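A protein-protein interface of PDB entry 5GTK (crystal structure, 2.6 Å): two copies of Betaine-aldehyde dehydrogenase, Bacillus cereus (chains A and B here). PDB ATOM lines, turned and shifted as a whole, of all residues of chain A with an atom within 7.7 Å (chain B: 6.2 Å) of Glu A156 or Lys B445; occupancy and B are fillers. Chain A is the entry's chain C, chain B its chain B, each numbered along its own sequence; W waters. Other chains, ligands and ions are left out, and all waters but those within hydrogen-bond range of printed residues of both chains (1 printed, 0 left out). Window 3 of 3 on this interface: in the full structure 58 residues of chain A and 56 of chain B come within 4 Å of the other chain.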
ATOM      1  N   ARG A  67      20.620 -15.291 -14.266  1.00  0.00           N
ATOM      2  CA  ARG A  67      20.058 -16.079 -13.159  1.00  0.00           C
ATOM      3  C   ARG A  67      20.505 -17.551 -13.229  1.00  0.00           C
ATOM      4  O   ARG A  67      20.863 -18.185 -12.218  1.00  0.00           O
ATOM      5  CB  ARG A  67      18.514 -15.979 -13.161  1.00  0.00           C
ATOM      6  CG  ARG A  67      17.795 -16.875 -12.158  1.00  0.00           C
ATOM      7  CD  ARG A  67      18.243 -16.648 -10.720  1.00  0.00           C
ATOM      8  NE  ARG A  67      17.977 -15.266 -10.370  1.00  0.00           N
ATOM      9  CZ  ARG A  67      18.502 -14.599  -9.342  1.00  0.00           C
ATOM     10  NH1 ARG A  67      19.348 -15.167  -8.508  1.00  0.00           N
ATOM     11  NH2 ARG A  67      18.162 -13.337  -9.146  1.00  0.00           N
ATOM     12  N   PHE A  70      24.176 -18.065 -12.474  1.00  0.00           N
ATOM     13  CA  PHE A  70      24.423 -17.925 -11.049  1.00  0.00           C
ATOM     14  C   PHE A  70      23.978 -19.133 -10.172  1.00  0.00           C
ATOM     15  O   PHE A  70      24.657 -19.478  -9.220  1.00  0.00           O
ATOM     16  CB  PHE A  70      23.790 -16.624 -10.515  1.00  0.00           C
ATOM     17  CG  PHE A  70      24.077 -16.366  -9.057  1.00  0.00           C
ATOM     18  CD1 PHE A  70      25.255 -15.774  -8.670  1.00  0.00           C
ATOM     19  CD2 PHE A  70      23.164 -16.724  -8.076  1.00  0.00           C
ATOM     20  CE1 PHE A  70      25.509 -15.527  -7.318  1.00  0.00           C
ATOM     21  CE2 PHE A  70      23.405 -16.483  -6.738  1.00  0.00           C
ATOM     22  CZ  PHE A  70      24.580 -15.906  -6.357  1.00  0.00           C
ATOM     23  N   GLU A  71      22.804 -19.691 -10.465  1.00  0.00           N
ATOM     24  CA  GLU A  71      22.233 -20.783  -9.704  1.00  0.00           C
ATOM     25  C   GLU A  71      22.874 -22.122 -10.072  1.00  0.00           C
ATOM     26  O   GLU A  71      22.900 -23.021  -9.264  1.00  0.00           O
ATOM     27  CB  GLU A  71      20.708 -20.861  -9.931  1.00  0.00           C
ATOM     28  CG  GLU A  71      19.885 -19.655  -9.488  1.00  0.00           C
ATOM     29  CD  GLU A  71      19.940 -19.380  -7.980  1.00  0.00           C
ATOM     30  OE1 GLU A  71      19.900 -18.174  -7.577  1.00  0.00           O
ATOM     31  OE2 GLU A  71      20.025 -20.360  -7.182  1.00  0.00           O
ATOM     32  N   ILE A 138      38.247 -12.606  -0.546  1.00  0.00           N
ATOM     33  CA  ILE A 138      37.048 -12.005  -0.037  1.00  0.00           C
ATOM     34  C   ILE A 138      36.612 -12.734   1.217  1.00  0.00           C
ATOM     35  O   ILE A 138      35.740 -13.515   1.196  1.00  0.00           O
ATOM     36  CB  ILE A 138      35.930 -11.983  -1.080  1.00  0.00           C
ATOM     37  CG1 ILE A 138      36.212 -10.940  -2.140  1.00  0.00           C
ATOM     38  CG2 ILE A 138      34.613 -11.596  -0.465  1.00  0.00           C
ATOM     39  CD1 ILE A 138      35.612 -11.289  -3.454  1.00  0.00           C
ATOM     40  N   THR A 153      30.758 -15.376   9.691  1.00  0.00           N
ATOM     41  CA  THR A 153      30.057 -14.699   8.636  1.00  0.00           C
ATOM     42  C   THR A 153      30.573 -15.145   7.285  1.00  0.00           C
ATOM     43  O   THR A 153      31.756 -15.412   7.115  1.00  0.00           O
ATOM     44  CB  THR A 153      30.153 -13.158   8.753  1.00  0.00           C
ATOM     45  OG1 THR A 153      31.502 -12.734   8.723  1.00  0.00           O
ATOM     46  CG2 THR A 153      29.530 -12.693  10.015  1.00  0.00           C
ATOM     47  N   ARG A 154      29.663 -15.249   6.332  1.00  0.00           N
ATOM     48  CA  ARG A 154      29.994 -15.517   4.930  1.00  0.00           C
ATOM     49  C   ARG A 154      29.639 -14.239   4.182  1.00  0.00           C
ATOM     50  O   ARG A 154      28.642 -13.603   4.477  1.00  0.00           O
ATOM     51  CB  ARG A 154      29.145 -16.668   4.366  1.00  0.00           C
ATOM     52  CG  ARG A 154      29.606 -18.078   4.668  1.00  0.00           C
ATOM     53  CD  ARG A 154      28.508 -19.148   4.450  1.00  0.00           C
ATOM     54  NE  ARG A 154      27.786 -19.155   3.152  1.00  0.00           N
ATOM     55  CZ  ARG A 154      28.171 -19.771   2.023  1.00  0.00           C
ATOM     56  NH1 ARG A 154      29.314 -20.425   1.948  1.00  0.00           N
ATOM     57  NH2 ARG A 154      27.410 -19.716   0.930  1.00  0.00           N
ATOM     58  N   HIS A 155      30.483 -13.853   3.240  1.00  0.00           N
ATOM     59  CA  HIS A 155      30.219 -12.750   2.309  1.00  0.00           C
ATOM     60  C   HIS A 155      29.773 -13.391   0.998  1.00  0.00           C
ATOM     61  O   HIS A 155      30.582 -13.769   0.184  1.00  0.00           O
ATOM     62  CB  HIS A 155      31.486 -11.932   2.158  1.00  0.00           C
ATOM     63  CG  HIS A 155      31.850 -11.159   3.400  1.00  0.00           C
ATOM     64  ND1 HIS A 155      32.676 -10.057   3.375  1.00  0.00           N
ATOM     65  CD2 HIS A 155      31.442 -11.284   4.686  1.00  0.00           C
ATOM     66  CE1 HIS A 155      32.811  -9.581   4.602  1.00  0.00           C
ATOM     67  NE2 HIS A 155      32.061 -10.299   5.411  1.00  0.00           N
ATOM     68  N   GLU A 156      28.471 -13.611   0.861  1.00  0.00           N
ATOM     69  CA  GLU A 156      27.933 -14.303  -0.303  1.00  0.00           C
ATOM     70  C   GLU A 156      27.710 -13.278  -1.424  1.00  0.00           C
ATOM     71  O   GLU A 156      27.221 -12.172  -1.158  1.00  0.00           O
ATOM     72  CB  GLU A 156      26.600 -14.994   0.045  1.00  0.00           C
ATOM     73  CG  GLU A 156      26.719 -16.107   1.079  1.00  0.00           C
ATOM     74  CD  GLU A 156      25.418 -16.814   1.390  1.00  0.00           C
ATOM     75  OE1 GLU A 156      24.363 -16.499   0.802  1.00  0.00           O
ATOM     76  OE2 GLU A 156      25.451 -17.733   2.218  1.00  0.00           O
ATOM     77  N   PRO A 157      28.024 -13.631  -2.671  1.00  0.00           N
ATOM     78  CA  PRO A 157      27.670 -12.690  -3.734  1.00  0.00           C
ATOM     79  C   PRO A 157      26.151 -12.442  -3.776  1.00  0.00           C
ATOM     80  O   PRO A 157      25.371 -13.406  -3.665  1.00  0.00           O
ATOM     81  CB  PRO A 157      28.155 -13.381  -5.014  1.00  0.00           C
ATOM     82  CG  PRO A 157      28.183 -14.826  -4.669  1.00  0.00           C
ATOM     83  CD  PRO A 157      28.527 -14.910  -3.206  1.00  0.00           C
ATOM     84  N   VAL A 158      25.739 -11.179  -3.919  1.00  0.00           N
ATOM     85  CA  VAL A 158      24.310 -10.802  -3.864  1.00  0.00           C
ATOM     86  C   VAL A 158      23.471 -11.441  -4.964  1.00  0.00           C
ATOM     87  O   VAL A 158      22.302 -11.743  -4.728  1.00  0.00           O
ATOM     88  CB  VAL A 158      24.102  -9.267  -3.759  1.00  0.00           C
ATOM     89  CG1 VAL A 158      24.549  -8.512  -5.015  1.00  0.00           C
ATOM     90  CG2 VAL A 158      22.658  -8.953  -3.410  1.00  0.00           C
ATOM     91  N   GLY A 159      24.071 -11.721  -6.129  1.00  0.00           N
ATOM     92  CA  GLY A 159      23.435 -12.543  -7.167  1.00  0.00           C
ATOM     93  C   GLY A 159      23.543 -11.931  -8.562  1.00  0.00           C
ATOM     94  O   GLY A 159      24.662 -11.677  -9.070  1.00  0.00           O
ATOM     95  N   THR A 184      33.408 -11.105  -6.672  1.00  0.00           N
ATOM     96  CA  THR A 184      32.556 -11.736  -5.650  1.00  0.00           C
ATOM     97  C   THR A 184      31.761 -12.950  -6.109  1.00  0.00           C
ATOM     98  O   THR A 184      31.209 -13.635  -5.267  1.00  0.00           O
ATOM     99  CB  THR A 184      31.554 -10.753  -5.017  1.00  0.00           C
ATOM    100  OG1 THR A 184      30.526 -10.379  -5.970  1.00  0.00           O
ATOM    101  CG2 THR A 184      32.303  -9.545  -4.462  1.00  0.00           C
ATOM    102  N   GLY A 185      31.674 -13.186  -7.425  1.00  0.00           N
ATOM    103  CA  GLY A 185      30.905 -14.299  -7.997  1.00  0.00           C
ATOM    104  C   GLY A 185      29.490 -13.980  -8.448  1.00  0.00           C
ATOM    105  O   GLY A 185      28.683 -14.890  -8.719  1.00  0.00           O
ATOM    106  N   CYS A 186      29.168 -12.693  -8.532  1.00  0.00           N
ATOM    107  CA  CYS A 186      27.913 -12.258  -9.118  1.00  0.00           C
ATOM    108  C   CYS A 186      27.871 -12.549 -10.632  1.00  0.00           C
ATOM    109  O   CYS A 186      28.885 -12.894 -11.256  1.00  0.00           O
ATOM    110  CB  CYS A 186      27.692 -10.770  -8.882  1.00  0.00           C
ATOM    111  SG  CYS A 186      27.463 -10.308  -7.158  1.00  0.00           S
ATOM    112  N   ASP A 238      19.012  -8.478  -8.384  1.00  0.00           N
ATOM    113  CA  ASP A 238      19.163  -8.421  -6.917  1.00  0.00           C
ATOM    114  C   ASP A 238      19.712  -7.130  -6.362  1.00  0.00           C
ATOM    115  O   ASP A 238      19.562  -6.868  -5.181  1.00  0.00           O
ATOM    116  CB  ASP A 238      20.022  -9.569  -6.418  1.00  0.00           C
ATOM    117  CG  ASP A 238      19.410 -10.930  -6.748  1.00  0.00           C
ATOM    118  OD1 ASP A 238      18.332 -11.299  -6.179  1.00  0.00           O
ATOM    119  OD2 ASP A 238      19.997 -11.640  -7.596  1.00  0.00           O
ATOM    120  N   LEU A 480      34.036  -4.170  -3.175  1.00  0.00           N
ATOM    121  CA  LEU A 480      33.543  -5.539  -3.005  1.00  0.00           C
ATOM    122  C   LEU A 480      32.256  -5.631  -2.216  1.00  0.00           C
ATOM    123  O   LEU A 480      31.378  -6.443  -2.520  1.00  0.00           O
ATOM    124  CB  LEU A 480      34.560  -6.405  -2.274  1.00  0.00           C
ATOM    125  CG  LEU A 480      35.880  -6.543  -3.008  1.00  0.00           C
ATOM    126  CD1 LEU A 480      36.896  -7.139  -2.044  1.00  0.00           C
ATOM    127  CD2 LEU A 480      35.673  -7.354  -4.290  1.00  0.00           C
ATOM    128  N   ASP A 481      32.179  -4.796  -1.195  1.00  0.00           N
ATOM    129  CA  ASP A 481      31.079  -4.801  -0.268  1.00  0.00           C
ATOM    130  C   ASP A 481      29.765  -4.493  -0.889  1.00  0.00           C
ATOM    131  O   ASP A 481      28.806  -4.957  -0.399  1.00  0.00           O
ATOM    132  CB  ASP A 481      31.370  -3.822   0.881  1.00  0.00           C
ATOM    133  CG  ASP A 481      32.583  -4.271   1.694  1.00  0.00           C
ATOM    134  OD1 ASP A 481      33.134  -5.363   1.350  1.00  0.00           O
ATOM    135  OD2 ASP A 481      32.971  -3.577   2.667  1.00  0.00           O
ATOM    136  N   TYR A 483      28.688  -5.814  -3.614  1.00  0.00           N
ATOM    137  CA  TYR A 483      28.207  -6.997  -4.279  1.00  0.00           C
ATOM    138  C   TYR A 483      28.090  -8.168  -3.380  1.00  0.00           C
ATOM    139  O   TYR A 483      28.055  -9.268  -3.768  1.00  0.00           O
ATOM    140  CB  TYR A 483      29.041  -7.289  -5.511  1.00  0.00           C
ATOM    141  CG  TYR A 483      29.040  -6.133  -6.401  1.00  0.00           C
ATOM    142  CD1 TYR A 483      27.928  -5.808  -7.117  1.00  0.00           C
ATOM    143  CD2 TYR A 483      30.121  -5.317  -6.481  1.00  0.00           C
ATOM    144  CE1 TYR A 483      27.908  -4.719  -7.904  1.00  0.00           C
ATOM    145  CE2 TYR A 483      30.091  -4.224  -7.261  1.00  0.00           C
ATOM    146  CZ  TYR A 483      28.965  -3.938  -7.977  1.00  0.00           C
ATOM    147  OH  TYR A 483      28.899  -2.864  -8.775  1.00  0.00           O
ATOM    148  N   THR A 484      28.006  -7.852  -2.125  1.00  0.00           N
ATOM    149  CA  THR A 484      27.970  -8.825  -1.099  1.00  0.00           C
ATOM    150  C   THR A 484      26.768  -8.812  -0.207  1.00  0.00           C
ATOM    151  O   THR A 484      26.152  -7.840   0.010  1.00  0.00           O
ATOM    152  CB  THR A 484      29.324  -8.719  -0.366  1.00  0.00           C
ATOM    153  OG1 THR A 484      30.209  -9.606  -0.970  1.00  0.00           O
ATOM    154  CG2 THR A 484      29.299  -9.048   1.037  1.00  0.00           C
ATOM    155  N   GLU A 485      26.466  -9.965   0.308  1.00  0.00           N
ATOM    156  CA  GLU A 485      25.394 -10.119   1.246  1.00  0.00           C
ATOM    157  C   GLU A 485      25.993 -10.871   2.431  1.00  0.00           C
ATOM    158  O   GLU A 485      26.449 -11.941   2.321  1.00  0.00           O
ATOM    159  CB  GLU A 485      24.201 -10.745   0.533  1.00  0.00           C
ATOM    160  CG  GLU A 485      22.854 -10.514   1.115  1.00  0.00           C
ATOM    161  CD  GLU A 485      22.322  -9.145   1.052  1.00  0.00           C
ATOM    162  OE1 GLU A 485      22.000  -8.653  -0.002  1.00  0.00           O
ATOM    163  OE2 GLU A 485      22.184  -8.568   2.073  1.00  0.00           O
ATOM    164  N   VAL A 486      26.045 -10.223   3.560  1.00  0.00           N
ATOM    165  CA  VAL A 486      26.640 -10.779   4.789  1.00  0.00           C
ATOM    166  C   VAL A 486      25.700 -11.754   5.439  1.00  0.00           C
ATOM    167  O   VAL A 486      24.602 -11.352   5.804  1.00  0.00           O
ATOM    168  CB  VAL A 486      26.931  -9.674   5.852  1.00  0.00           C
ATOM    169  CG1 VAL A 486      27.421 -10.272   7.165  1.00  0.00           C
ATOM    170  CG2 VAL A 486      27.942  -8.673   5.313  1.00  0.00           C
ATOM    171  N   LYS A 487      26.135 -12.998   5.608  1.00  0.00           N
ATOM    172  CA  LYS A 487      25.369 -14.026   6.312  1.00  0.00           C
ATOM    173  C   LYS A 487      26.109 -14.282   7.642  1.00  0.00           C
ATOM    174  O   LYS A 487      27.315 -14.535   7.644  1.00  0.00           O
ATOM    175  CB  LYS A 487      25.222 -15.325   5.478  1.00  0.00           C
ATOM    176  CG  LYS A 487      24.345 -16.407   6.154  1.00  0.00           C
ATOM    177  CD  LYS A 487      24.077 -17.677   5.353  1.00  0.00           C
ATOM    178  CE  LYS A 487      23.151 -17.412   4.161  1.00  0.00           C
ATOM    179  NZ  LYS A 487      23.098 -18.554   3.175  1.00  0.00           N
ATOM    180  N   SER A 488      25.376 -14.192   8.754  1.00  0.00           N
ATOM    181  CA  SER A 488      25.866 -14.542  10.083  1.00  0.00           C
ATOM    182  C   SER A 488      25.311 -15.909  10.487  1.00  0.00           C
ATOM    183  O   SER A 488      24.095 -16.082  10.571  1.00  0.00           O
ATOM    184  CB  SER A 488      25.422 -13.507  11.118  1.00  0.00           C
ATOM    185  OG  SER A 488      25.882 -13.871  12.420  1.00  0.00           O
ATOM    186  N   VAL A 489      26.211 -16.854  10.750  1.00  0.00           N
ATOM    187  CA  VAL A 489      25.843 -18.228  11.048  1.00  0.00           C
ATOM    188  C   VAL A 489      26.255 -18.506  12.472  1.00  0.00           C
ATOM    189  O   VAL A 489      27.386 -18.204  12.868  1.00  0.00           O
ATOM    190  CB  VAL A 489      26.561 -19.231  10.099  1.00  0.00           C
ATOM    191  CG1 VAL A 489      26.107 -20.652  10.363  1.00  0.00           C
ATOM    192  CG2 VAL A 489      26.288 -18.864   8.642  1.00  0.00           C
ATOM    193  N   ASN B 419      12.963 -20.521   0.933  1.00  0.00           N
ATOM    194  CA  ASN B 419      13.447 -19.474   0.117  1.00  0.00           C
ATOM    195  C   ASN B 419      12.413 -18.749  -0.714  1.00  0.00           C
ATOM    196  O   ASN B 419      12.653 -17.683  -1.118  1.00  0.00           O
ATOM    197  CB  ASN B 419      14.567 -19.988  -0.745  1.00  0.00           C
ATOM    198  CG  ASN B 419      15.879 -20.072  -0.033  1.00  0.00           C
ATOM    199  OD1 ASN B 419      16.058 -19.590   1.032  1.00  0.00           O
ATOM    200  ND2 ASN B 419      16.803 -20.663  -0.671  1.00  0.00           N
ATOM    201  N   TYR B 423      10.871 -12.130   1.971  1.00  0.00           N
ATOM    202  CA  TYR B 423      11.657 -11.910   3.131  1.00  0.00           C
ATOM    203  C   TYR B 423      12.902 -12.754   3.194  1.00  0.00           C
ATOM    204  O   TYR B 423      13.012 -13.753   2.592  1.00  0.00           O
ATOM    205  CB  TYR B 423      10.832 -12.265   4.354  1.00  0.00           C
ATOM    206  CG  TYR B 423       9.714 -11.373   4.610  1.00  0.00           C
ATOM    207  CD1 TYR B 423       9.929 -10.056   4.766  1.00  0.00           C
ATOM    208  CD2 TYR B 423       8.445 -11.834   4.669  1.00  0.00           C
ATOM    209  CE1 TYR B 423       8.924  -9.208   5.003  1.00  0.00           C
ATOM    210  CE2 TYR B 423       7.415 -10.990   4.896  1.00  0.00           C
ATOM    211  CZ  TYR B 423       7.684  -9.679   5.073  1.00  0.00           C
ATOM    212  OH  TYR B 423       6.693  -8.823   5.287  1.00  0.00           O
ATOM    213  N   GLY B 424      13.845 -12.319   3.968  1.00  0.00           N
ATOM    214  CA  GLY B 424      15.043 -13.134   4.156  1.00  0.00           C
ATOM    215  C   GLY B 424      15.874 -12.584   5.290  1.00  0.00           C
ATOM    216  O   GLY B 424      17.027 -12.186   5.104  1.00  0.00           O
ATOM    217  N   LEU B 425      15.261 -12.543   6.473  1.00  0.00           N
ATOM    218  CA  LEU B 425      15.864 -11.895   7.627  1.00  0.00           C
ATOM    219  C   LEU B 425      16.653 -12.864   8.474  1.00  0.00           C
ATOM    220  O   LEU B 425      17.797 -12.562   8.837  1.00  0.00           O
ATOM    221  CB  LEU B 425      14.793 -11.275   8.480  1.00  0.00           C
ATOM    222  CG  LEU B 425      15.312 -10.502   9.671  1.00  0.00           C
ATOM    223  CD1 LEU B 425      16.329  -9.458   9.197  1.00  0.00           C
ATOM    224  CD2 LEU B 425      14.124  -9.862  10.355  1.00  0.00           C
ATOM    225  N   ALA B 426      16.032 -14.011   8.795  1.00  0.00           N
ATOM    226  CA  ALA B 426      16.647 -15.043   9.603  1.00  0.00           C
ATOM    227  C   ALA B 426      16.159 -16.428   9.234  1.00  0.00           C
ATOM    228  O   ALA B 426      15.232 -16.591   8.462  1.00  0.00           O
ATOM    229  CB  ALA B 426      16.394 -14.773  11.075  1.00  0.00           C
ATOM    230  N   ALA B 441      22.495 -24.183   5.780  1.00  0.00           N
ATOM    231  CA  ALA B 441      22.871 -22.791   6.111  1.00  0.00           C
ATOM    232  C   ALA B 441      23.327 -21.992   4.901  1.00  0.00           C
ATOM    233  O   ALA B 441      22.898 -20.851   4.717  1.00  0.00           O
ATOM    234  CB  ALA B 441      23.945 -22.734   7.203  1.00  0.00           C
ATOM    235  N   ASN B 442      24.174 -22.608   4.080  1.00  0.00           N
ATOM    236  CA  ASN B 442      24.709 -21.963   2.851  1.00  0.00           C
ATOM    237  C   ASN B 442      23.660 -21.614   1.835  1.00  0.00           C
ATOM    238  O   ASN B 442      23.698 -20.548   1.263  1.00  0.00           O
ATOM    239  CB  ASN B 442      25.782 -22.834   2.180  1.00  0.00           C
ATOM    240  CG  ASN B 442      27.134 -22.848   2.931  1.00  0.00           C
ATOM    241  OD1 ASN B 442      28.041 -23.519   2.458  1.00  0.00           O
ATOM    242  ND2 ASN B 442      27.282 -22.158   4.067  1.00  0.00           N
ATOM    243  N   LYS B 443      22.697 -22.507   1.668  1.00  0.00           N
ATOM    244  CA  LYS B 443      21.646 -22.357   0.671  1.00  0.00           C
ATOM    245  C   LYS B 443      20.450 -21.448   1.064  1.00  0.00           C
ATOM    246  O   LYS B 443      19.748 -20.990   0.178  1.00  0.00           O
ATOM    247  CB  LYS B 443      21.131 -23.749   0.239  1.00  0.00           C
ATOM    248  CG  LYS B 443      21.728 -24.285  -1.059  1.00  0.00           C
ATOM    249  CD  LYS B 443      22.855 -25.294  -0.845  1.00  0.00           C
ATOM    250  CE  LYS B 443      22.318 -26.728  -0.874  1.00  0.00           C
ATOM    251  NZ  LYS B 443      22.085 -27.203  -2.270  1.00  0.00           N
ATOM    252  N   LEU B 444      20.218 -21.150   2.320  1.00  0.00           N
ATOM    253  CA  LEU B 444      19.134 -20.296   2.693  1.00  0.00           C
ATOM    254  C   LEU B 444      19.399 -18.822   2.516  1.00  0.00           C
ATOM    255  O   LEU B 444      20.362 -18.297   2.971  1.00  0.00           O
ATOM    256  CB  LEU B 444      18.699 -20.548   4.118  1.00  0.00           C
ATOM    257  CG  LEU B 444      18.076 -21.853   4.475  1.00  0.00           C
ATOM    258  CD1 LEU B 444      18.113 -22.129   5.924  1.00  0.00           C
ATOM    259  CD2 LEU B 444      16.751 -22.170   3.853  1.00  0.00           C
ATOM    260  N   LYS B 445      18.498 -18.145   1.854  1.00  0.00           N
ATOM    261  CA  LYS B 445      18.615 -16.737   1.613  1.00  0.00           C
ATOM    262  C   LYS B 445      18.141 -15.961   2.837  1.00  0.00           C
ATOM    263  O   LYS B 445      17.032 -15.560   2.904  1.00  0.00           O
ATOM    264  CB  LYS B 445      17.835 -16.391   0.366  1.00  0.00           C
ATOM    265  CG  LYS B 445      18.626 -16.333  -0.884  1.00  0.00           C
ATOM    266  CD  LYS B 445      19.253 -17.646  -1.287  1.00  0.00           C
ATOM    267  CE  LYS B 445      20.713 -17.529  -1.698  1.00  0.00           C
ATOM    268  NZ  LYS B 445      21.741 -17.994  -0.718  1.00  0.00           N
ATOM    269  N   ALA B 446      19.022 -15.774   3.801  1.00  0.00           N
ATOM    270  CA  ALA B 446      18.738 -15.154   5.084  1.00  0.00           C
ATOM    271  C   ALA B 446      19.977 -14.587   5.713  1.00  0.00           C
ATOM    272  O   ALA B 446      21.007 -15.162   5.673  1.00  0.00           O
ATOM    273  CB  ALA B 446      18.138 -16.159   6.023  1.00  0.00           C
ATOM    274  N   GLY B 447      19.828 -13.436   6.328  1.00  0.00           N
ATOM    275  CA  GLY B 447      20.901 -12.720   6.977  1.00  0.00           C
ATOM    276  C   GLY B 447      21.544 -13.403   8.123  1.00  0.00           C
ATOM    277  O   GLY B 447      22.687 -13.254   8.324  1.00  0.00           O
ATOM    278  N   TYR B 466      18.201  -9.974   3.756  1.00  0.00           N
ATOM    279  CA  TYR B 466      18.418 -10.234   2.347  1.00  0.00           C
ATOM    280  C   TYR B 466      17.076  -9.834   1.820  1.00  0.00           C
ATOM    281  O   TYR B 466      16.152  -9.834   2.542  1.00  0.00           O
ATOM    282  CB  TYR B 466      18.548 -11.728   2.036  1.00  0.00           C
ATOM    283  CG  TYR B 466      19.871 -12.393   2.157  1.00  0.00           C
ATOM    284  CD1 TYR B 466      20.689 -12.133   3.177  1.00  0.00           C
ATOM    285  CD2 TYR B 466      20.263 -13.326   1.248  1.00  0.00           C
ATOM    286  CE1 TYR B 466      21.885 -12.752   3.285  1.00  0.00           C
ATOM    287  CE2 TYR B 466      21.438 -13.966   1.356  1.00  0.00           C
ATOM    288  CZ  TYR B 466      22.239 -13.654   2.387  1.00  0.00           C
ATOM    289  OH  TYR B 466      23.403 -14.245   2.539  1.00  0.00           O
ATOM    290  N   LYS B 467      16.963  -9.513   0.550  1.00  0.00           N
ATOM    291  CA  LYS B 467      15.680  -9.143  -0.047  1.00  0.00           C
ATOM    292  C   LYS B 467      14.852  -8.025   0.597  1.00  0.00           C
ATOM    293  O   LYS B 467      15.352  -6.999   0.803  1.00  0.00           O
ATOM    294  CB  LYS B 467      14.809 -10.360  -0.317  1.00  0.00           C
ATOM    295  CG  LYS B 467      15.448 -11.495  -1.044  1.00  0.00           C
ATOM    296  CD  LYS B 467      14.988 -12.761  -0.415  1.00  0.00           C
ATOM    297  CE  LYS B 467      14.825 -13.880  -1.381  1.00  0.00           C
ATOM    298  NZ  LYS B 467      13.940 -14.912  -0.835  1.00  0.00           N
HETATM  299  O   HOH W   1      24.177 -10.906   9.087  1.00  0.00           O
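OE2 of Glu A156 lies close to O of Asn B442 (3.5 Å). The guanidinium group (NE) of Arg A154 lies close to the side-chain amide nitrogen (ND2) of Asn B442. The backbone carbonyl oxygen (O) of Ala B441 is in hydrogen-bond range of the side-chain amino group (NZ) of Lys A487 (2.8 Å). NZ of Lys A487 is in hydrogen-bond range of O of Leu B444. The side-chain carboxylate (OE1) of Glu A156 lies within hydrogen-bond range of the side-chain hydroxyl (OH) of Tyr B466, at 3.0 Å. O of Asn B442 lies within hydrogen-bond range of NZ of Lys A487 (2.8 Å). O of Gly B447 lies within hydrogen-bond range of N of Ser A488 (2.9 Å). OE1 of Glu A156 is in salt-bridge range of NZ of Lys B445 (3.4 Å).
The side-chain carboxylate (OE2) of Glu A156 lies within salt-bridge range of the side-chain amino group (NZ) of Lys A487 (2.7 Å). The backbone carbonyl oxygen of Gly B424 lies within hydrogen-bond range of the backbone NH of Gly B447 (3.3 Å). O of Gly B424 lies within hydrogen-bond range of N of Tyr B466 (2.8 Å). The backbone carbonyl oxygen (O) of Lys A487 sits at hydrogen-bond distance from the backbone NH (N) of Arg A154. The guanidinium group (NE) of Arg A154 is in salt-bridge range of the side-chain carboxylate (OE2) of Glu A156. The backbone NH (N) of Lys B445 sits at hydrogen-bond distance from the side-chain amide oxygen (OD1) of Asn B419 (3.0 Å).
Among the printed residues, merely in contact across the chains: Glu A485 with Tyr B466, Val A486 with Gly B447, Val A486 with Tyr B466, Lys A487 with Ala B446, Lys A487 with Gly B447 and Lys A487 with Tyr B466.
Of chain B, only Asn B442 (3.5 Å), Lys B445 (3.4 Å) and Tyr B466 (3.0 Å) come within 4 Å of Glu A156. Of chain A, only Glu A156 (3.4 Å) comes within 4 Å of Lys B445. Of the printed residues of chain A, Asn B442 touches Arg A154 (3.2 Å), Glu A156 (3.5 Å) and Lys A487 (2.8 Å). Of the printed residues of chain A, Ala B446 touches Lys A487. Of the printed residues of chain B, Ser A488 touches Gly B447. Printed residues of chain B within 4 Å of Lys A487: Ala B441, Asn B442, Leu B444, Ala B446, Gly B447 and Tyr B466. Glu A71 touches none of the printed residues of chain B. The nearest residue of chain B that does not touch Glu A156 is Ala B441 (4.7 Å). The nearest residue of chain A that does not touch Lys B445 is Lys A487 (4.2 Å).
Printed residues of chain B that touch a printed residue of chain A: Ala B441, Asn B442, Leu B444, Lys B445, Ala B446, Gly B447 and Tyr B466. Hydrophobic or aromatic side chains of chain B that line the printed part of chain A: Tyr B466. Of the 24 printed residues of chain A, 6 touch a printed residue of chain B. Among the printed residues, 14 pairs touch across the chains. Among the printed residues, Asp or Glu carboxylates within 4 Å of a Lys or Arg side-chain nitrogen of the other chain: Glu A156 with Lys B445 (3.4 Å).
No position is printed for both chains. Of the 14 pairs that touch across the chains among the printed residues, none has its exchanged pair printed and touching as well.
Water W1 bridges O of Gly B447 (2.9 Å) and O of Val A486 (3.3 Å).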
